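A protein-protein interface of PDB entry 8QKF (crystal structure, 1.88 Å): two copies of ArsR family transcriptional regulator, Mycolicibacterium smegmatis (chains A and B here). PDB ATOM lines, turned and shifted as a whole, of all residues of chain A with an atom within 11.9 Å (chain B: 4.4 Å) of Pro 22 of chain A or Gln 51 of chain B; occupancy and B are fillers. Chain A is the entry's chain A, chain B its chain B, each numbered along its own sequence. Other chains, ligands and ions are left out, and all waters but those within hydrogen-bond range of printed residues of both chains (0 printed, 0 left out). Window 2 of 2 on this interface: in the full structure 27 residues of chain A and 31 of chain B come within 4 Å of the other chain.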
ATOM      1  N   PRO A  20       5.475   0.574 -18.518  1.00  0.00           N
ATOM      2  CA  PRO A  20       4.627   1.741 -18.272  1.00  0.00           C
ATOM      3  C   PRO A  20       3.709   1.593 -17.009  1.00  0.00           C
ATOM      4  O   PRO A  20       4.193   1.789 -15.872  1.00  0.00           O
ATOM      5  CB  PRO A  20       3.843   1.865 -19.594  1.00  0.00           C
ATOM      6  CG  PRO A  20       3.749   0.454 -20.125  1.00  0.00           C
ATOM      7  CD  PRO A  20       4.867  -0.352 -19.496  1.00  0.00           C
ATOM      8  N   ALA A  21       2.421   1.263 -17.215  1.00  0.00           N
ATOM      9  CA  ALA A  21       1.410   1.089 -16.145  1.00  0.00           C
ATOM     10  C   ALA A  21       1.229  -0.416 -15.863  1.00  0.00           C
ATOM     11  O   ALA A  21       0.920  -1.155 -16.804  1.00  0.00           O
ATOM     12  CB  ALA A  21       0.069   1.680 -16.581  1.00  0.00           C
ATOM     13  N   PRO A  22       1.400  -0.870 -14.583  1.00  0.00           N
ATOM     14  CA  PRO A  22       1.233  -2.314 -14.205  1.00  0.00           C
ATOM     15  C   PRO A  22      -0.252  -2.755 -14.524  1.00  0.00           C
ATOM     16  O   PRO A  22      -1.125  -1.870 -14.617  1.00  0.00           O
ATOM     17  CB  PRO A  22       1.698  -2.347 -12.740  1.00  0.00           C
ATOM     18  CG  PRO A  22       1.502  -0.952 -12.226  1.00  0.00           C
ATOM     19  CD  PRO A  22       1.584  -0.002 -13.396  1.00  0.00           C
ATOM     20  N   ALA A  23      -0.611  -4.039 -14.687  1.00  0.00           N
ATOM     21  CA  ALA A  23      -0.801  -5.113 -13.667  1.00  0.00           C
ATOM     22  C   ALA A  23      -2.319  -5.029 -13.400  1.00  0.00           C
ATOM     23  O   ALA A  23      -3.086  -5.377 -14.297  1.00  0.00           O
ATOM     24  CB  ALA A  23       0.040  -5.045 -12.382  1.00  0.00           C
ATOM     25  N   LEU A  24      -2.758  -4.464 -12.274  1.00  0.00           N
ATOM     26  CA  LEU A  24      -4.026  -4.859 -11.609  1.00  0.00           C
ATOM     27  C   LEU A  24      -3.783  -6.330 -11.244  1.00  0.00           C
ATOM     28  O   LEU A  24      -3.620  -7.184 -12.117  1.00  0.00           O
ATOM     29  CB  LEU A  24      -5.342  -4.700 -12.449  1.00  0.00           C
ATOM     30  CG  LEU A  24      -6.158  -3.383 -12.590  1.00  0.00           C
ATOM     31  CD1 LEU A  24      -7.582  -3.561 -13.135  1.00  0.00           C
ATOM     32  CD2 LEU A  24      -6.259  -2.643 -11.274  1.00  0.00           C
ATOM     33  N   PRO A  25      -3.660  -6.618  -9.953  1.00  0.00           N
ATOM     34  CA  PRO A  25      -3.846  -8.013  -9.534  1.00  0.00           C
ATOM     35  C   PRO A  25      -5.339  -8.372  -9.768  1.00  0.00           C
ATOM     36  O   PRO A  25      -6.109  -7.445 -10.076  1.00  0.00           O
ATOM     37  CB  PRO A  25      -3.461  -7.974  -8.053  1.00  0.00           C
ATOM     38  CG  PRO A  25      -2.590  -6.744  -7.908  1.00  0.00           C
ATOM     39  CD  PRO A  25      -3.117  -5.753  -8.890  1.00  0.00           C
ATOM     40  N   SER A  26      -5.746  -9.660  -9.688  1.00  0.00           N
ATOM     41  CA  SER A  26      -7.202 -10.055  -9.595  1.00  0.00           C
ATOM     42  C   SER A  26      -7.663  -9.087  -8.543  1.00  0.00           C
ATOM     43  O   SER A  26      -6.921  -8.919  -7.589  1.00  0.00           O
ATOM     44  CB  SER A  26      -7.334 -11.498  -9.157  1.00  0.00           C
ATOM     45  OG  SER A  26      -6.504 -11.760  -8.036  1.00  0.00           O
ATOM     46  N   ARG A  27      -8.843  -8.476  -8.580  1.00  0.00           N
ATOM     47  CA  ARG A  27     -10.096  -8.921  -8.026  1.00  0.00           C
ATOM     48  C   ARG A  27      -9.922  -9.626  -6.699  1.00  0.00           C
ATOM     49  O   ARG A  27     -10.093  -8.989  -5.659  1.00  0.00           O
ATOM     50  CB  ARG A  27     -11.072  -9.579  -8.991  1.00  0.00           C
ATOM     51  CG  ARG A  27     -12.490  -9.008  -8.820  1.00  0.00           C
ATOM     52  CD  ARG A  27     -12.517  -7.475  -8.988  1.00  0.00           C
ATOM     53  NE  ARG A  27     -13.854  -6.864  -8.961  1.00  0.00           N
ATOM     54  CZ  ARG A  27     -14.747  -6.916  -9.949  1.00  0.00           C
ATOM     55  NH1 ARG A  27     -14.493  -7.582 -11.073  1.00  0.00           N
ATOM     56  NH2 ARG A  27     -15.920  -6.310  -9.804  1.00  0.00           N
ATOM     57  N   LEU A  30      -7.065  -8.140  -4.600  1.00  0.00           N
ATOM     58  CA  LEU A  30      -7.309  -6.765  -4.226  1.00  0.00           C
ATOM     59  C   LEU A  30      -8.286  -6.703  -3.090  1.00  0.00           C
ATOM     60  O   LEU A  30      -8.138  -5.879  -2.174  1.00  0.00           O
ATOM     61  CB  LEU A  30      -7.853  -5.927  -5.375  1.00  0.00           C
ATOM     62  CG  LEU A  30      -6.888  -5.444  -6.471  1.00  0.00           C
ATOM     63  CD1 LEU A  30      -7.721  -4.645  -7.470  1.00  0.00           C
ATOM     64  CD2 LEU A  30      -5.725  -4.601  -5.956  1.00  0.00           C
ATOM     65  N   ALA B  47      -5.694  -0.003  -6.154  1.00  0.00           N
ATOM     66  CA  ALA B  47      -5.363  -0.021  -7.573  1.00  0.00           C
ATOM     67  C   ALA B  47      -4.812   1.347  -7.998  1.00  0.00           C
ATOM     68  O   ALA B  47      -3.877   1.416  -8.740  1.00  0.00           O
ATOM     69  CB  ALA B  47      -6.605  -0.372  -8.394  1.00  0.00           C
ATOM     70  N   ILE B  48      -5.393   2.405  -7.460  1.00  0.00           N
ATOM     71  CA  ILE B  48      -4.945   3.771  -7.747  1.00  0.00           C
ATOM     72  C   ILE B  48      -3.541   3.999  -7.232  1.00  0.00           C
ATOM     73  O   ILE B  48      -2.671   4.474  -7.969  1.00  0.00           O
ATOM     74  CB  ILE B  48      -5.937   4.810  -7.215  1.00  0.00           C
ATOM     75  CG1 ILE B  48      -7.247   4.767  -8.022  1.00  0.00           C
ATOM     76  CG2 ILE B  48      -5.330   6.215  -7.247  1.00  0.00           C
ATOM     77  CD1 ILE B  48      -8.322   5.762  -7.592  1.00  0.00           C
ATOM     78  N   VAL B  49      -3.281   3.557  -6.009  1.00  0.00           N
ATOM     79  CA  VAL B  49      -1.989   3.716  -5.406  1.00  0.00           C
ATOM     80  C   VAL B  49      -0.906   2.953  -6.142  1.00  0.00           C
ATOM     81  O   VAL B  49       0.224   3.446  -6.309  1.00  0.00           O
ATOM     82  CB  VAL B  49      -2.066   3.322  -3.898  1.00  0.00           C
ATOM     83  CG1 VAL B  49      -0.697   3.194  -3.280  1.00  0.00           C
ATOM     84  CG2 VAL B  49      -2.865   4.364  -3.161  1.00  0.00           C
ATOM     85  N   LEU B  50      -1.188   1.721  -6.542  1.00  0.00           N
ATOM     86  CA  LEU B  50      -0.193   0.986  -7.330  1.00  0.00           C
ATOM     87  C   LEU B  50       0.123   1.657  -8.678  1.00  0.00           C
ATOM     88  O   LEU B  50       1.216   1.560  -9.157  1.00  0.00           O
ATOM     89  CB  LEU B  50      -0.712  -0.399  -7.652  1.00  0.00           C
ATOM     90  CG  LEU B  50      -0.833  -1.300  -6.430  1.00  0.00           C
ATOM     91  CD1 LEU B  50      -1.645  -2.517  -6.855  1.00  0.00           C
ATOM     92  CD2 LEU B  50       0.547  -1.679  -5.926  1.00  0.00           C
ATOM     93  N   GLN B  51      -0.853   2.280  -9.286  1.00  0.00           N
ATOM     94  CA  GLN B  51      -0.571   3.064 -10.535  1.00  0.00           C
ATOM     95  C   GLN B  51       0.336   4.301 -10.264  1.00  0.00           C
ATOM     96  O   GLN B  51       1.298   4.565 -10.955  1.00  0.00           O
ATOM     97  CB  GLN B  51      -1.888   3.584 -11.127  1.00  0.00           C
ATOM     98  CG  GLN B  51      -2.798   2.532 -11.772  1.00  0.00           C
ATOM     99  CD  GLN B  51      -2.107   1.796 -12.898  1.00  0.00           C
ATOM    100  OE1 GLN B  51      -1.602   2.429 -13.852  1.00  0.00           O
ATOM    101  NE2 GLN B  51      -2.063   0.450 -12.795  1.00  0.00           N
ATOM    102  N   LEU B  52      -0.016   5.055  -9.236  1.00  0.00           N
ATOM    103  CA  LEU B  52       0.733   6.235  -8.822  1.00  0.00           C
ATOM    104  C   LEU B  52       2.082   5.916  -8.267  1.00  0.00           C
ATOM    105  O   LEU B  52       2.978   6.748  -8.265  1.00  0.00           O
ATOM    106  CB  LEU B  52      -0.059   7.077  -7.828  1.00  0.00           C
ATOM    107  CG  LEU B  52      -1.325   7.555  -8.479  1.00  0.00           C
ATOM    108  CD1 LEU B  52      -2.065   8.394  -7.446  1.00  0.00           C
ATOM    109  CD2 LEU B  52      -1.092   8.343  -9.780  1.00  0.00           C
ATOM    110  N   LYS B  53       2.290   4.706  -7.823  1.00  0.00           N
ATOM    111  CA  LYS B  53       3.610   4.389  -7.349  1.00  0.00           C
ATOM    112  C   LYS B  53       4.631   4.432  -8.500  1.00  0.00           C
ATOM    113  O   LYS B  53       5.796   4.781  -8.306  1.00  0.00           O
ATOM    114  CB  LYS B  53       3.544   3.002  -6.737  1.00  0.00           C
ATOM    115  CG  LYS B  53       4.855   2.262  -6.623  1.00  0.00           C
ATOM    116  CD  LYS B  53       4.580   0.755  -6.437  1.00  0.00           C
ATOM    117  CE  LYS B  53       5.679   0.209  -5.622  1.00  0.00           C
ATOM    118  NZ  LYS B  53       6.454   1.211  -4.820  1.00  0.00           N
ATOM    119  N   GLN B  54       4.211   4.090  -9.705  1.00  0.00           N
ATOM    120  CA  GLN B  54       5.133   4.041 -10.855  1.00  0.00           C
ATOM    121  C   GLN B  54       5.368   5.427 -11.499  1.00  0.00           C
ATOM    122  O   GLN B  54       6.457   5.740 -12.016  1.00  0.00           O
ATOM    123  CB  GLN B  54       4.594   3.028 -11.903  1.00  0.00           C
ATOM    124  CG  GLN B  54       4.502   1.574 -11.387  1.00  0.00           C
ATOM    125  CD  GLN B  54       5.805   1.095 -10.726  1.00  0.00           C
ATOM    126  OE1 GLN B  54       5.806   0.540  -9.614  1.00  0.00           O
ATOM    127  NE2 GLN B  54       6.929   1.369 -11.383  1.00  0.00           N
ATOM    128  N   SER B  55       4.354   6.264 -11.444  1.00  0.00           N
ATOM    129  CA  SER B  55       4.384   7.490 -12.177  1.00  0.00           C
ATOM    130  C   SER B  55       3.175   8.338 -11.762  1.00  0.00           C
ATOM    131  O   SER B  55       2.079   7.810 -11.493  1.00  0.00           O
ATOM    132  CB  SER B  55       4.350   7.180 -13.714  1.00  0.00           C
ATOM    133  OG  SER B  55       3.787   8.268 -14.486  1.00  0.00           O
ATOM    134  N   LEU B  62      -5.586   6.963 -15.621  1.00  0.00           N
ATOM    135  CA  LEU B  62      -6.010   6.019 -14.550  1.00  0.00           C
ATOM    136  C   LEU B  62      -7.277   5.299 -14.980  1.00  0.00           C
ATOM    137  O   LEU B  62      -7.390   4.088 -14.819  1.00  0.00           O
ATOM    138  CB  LEU B  62      -6.244   6.725 -13.208  1.00  0.00           C
ATOM    139  CG  LEU B  62      -5.027   7.380 -12.481  1.00  0.00           C
ATOM    140  CD1 LEU B  62      -5.511   8.272 -11.341  1.00  0.00           C
ATOM    141  CD2 LEU B  62      -4.025   6.355 -11.995  1.00  0.00           C
ATOM    142  N   ALA B  65      -6.057   2.507 -17.396  1.00  0.00           N
ATOM    143  CA  ALA B  65      -5.356   1.400 -16.697  1.00  0.00           C
ATOM    144  C   ALA B  65      -6.236   0.543 -15.771  1.00  0.00           C
ATOM    145  O   ALA B  65      -5.932  -0.619 -15.530  1.00  0.00           O
ATOM    146  CB  ALA B  65      -4.198   1.960 -15.885  1.00  0.00           C
ATOM    147  N   LEU B  66      -7.269   1.167 -15.222  1.00  0.00           N
ATOM    148  CA  LEU B  66      -8.193   0.567 -14.269  1.00  0.00           C
ATOM    149  C   LEU B  66      -9.465   0.011 -14.913  1.00  0.00           C
ATOM    150  O   LEU B  66     -10.129  -0.840 -14.316  1.00  0.00           O
ATOM    151  CB  LEU B  66      -8.665   1.617 -13.247  1.00  0.00           C
ATOM    152  CG  LEU B  66      -7.645   2.298 -12.303  1.00  0.00           C
ATOM    153  CD1 LEU B  66      -8.367   2.876 -11.104  1.00  0.00           C
ATOM    154  CD2 LEU B  66      -6.543   1.344 -11.881  1.00  0.00           C
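Of chain B, only Leu 50 (3.98 Å), Gln 51 (3.1 Å) and Gln 54 (3.9 Å) come within 4 Å of Pro 22 of chain A.
No residue of chain A comes within 4 Å of Ile 48 of chain B.
Gln 54 of chain B touches just one residue of chain A: Pro 22 (3.9 Å).
Ser 55 of chain B touches none of the printed residues of chain A.
No residue of chain A comes within 4 Å of Leu 62 of chain B.
No residue of chain A comes within 4 Å of Ala 65 of chain B.
Of the printed residues of chain B, Leu 24 of chain A touches Ala 47 (3.7 Å) and Leu 66 (3.9 Å).
Of the printed residues of chain A, Leu 66 of chain B touches Leu 24.
Of the printed residues of chain B, Ala 21 of chain A touches Gln 51.
The nearest printed residue of chain A that does not touch Leu 66 of chain B is Pro 22 of chain A (6.9 Å).
O of Pro 22 of chain A is in hydrogen-bond range of NE2 of Gln 51 of chain B (3.1 Å).
Gln 51 of chain B touches Ala 21 of chain A (OE1 to CB, 3.3 Å).
Pro 22 of chain A touches Leu 50 of chain B.
Gln 54 of chain B touches Pro 22 of chain A (CG to CD, 3.9 Å).
CD2 of Leu 24 of chain A touches CB of Ala 47 of chain B, 3.7 Å away.
Leu 66 of chain B touches Leu 24 of chain A.
Of the 12 printed residues of chain B, 5 touch a printed residue of chain A.
Hydrophobic or aromatic side chains of chain B within 4 Å of the printed part of chain A: Ala 47.
Printed residues of chain A that touch a printed residue of chain B: Ala 21, Pro 22 and Leu 24.
Hydrophobic or aromatic side chains of chain A within 4 Å of the printed part of chain B: Ala 21, Pro 22 and Leu 24.
Along chain A the printed residues that touch a printed residue of chain B span positions 21 to 24.
Among the printed residues, no Asp or Glu carboxylate lies within 4 Å of a Lys or Arg side-chain nitrogen of the other chain.
No position is printed for both chains.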
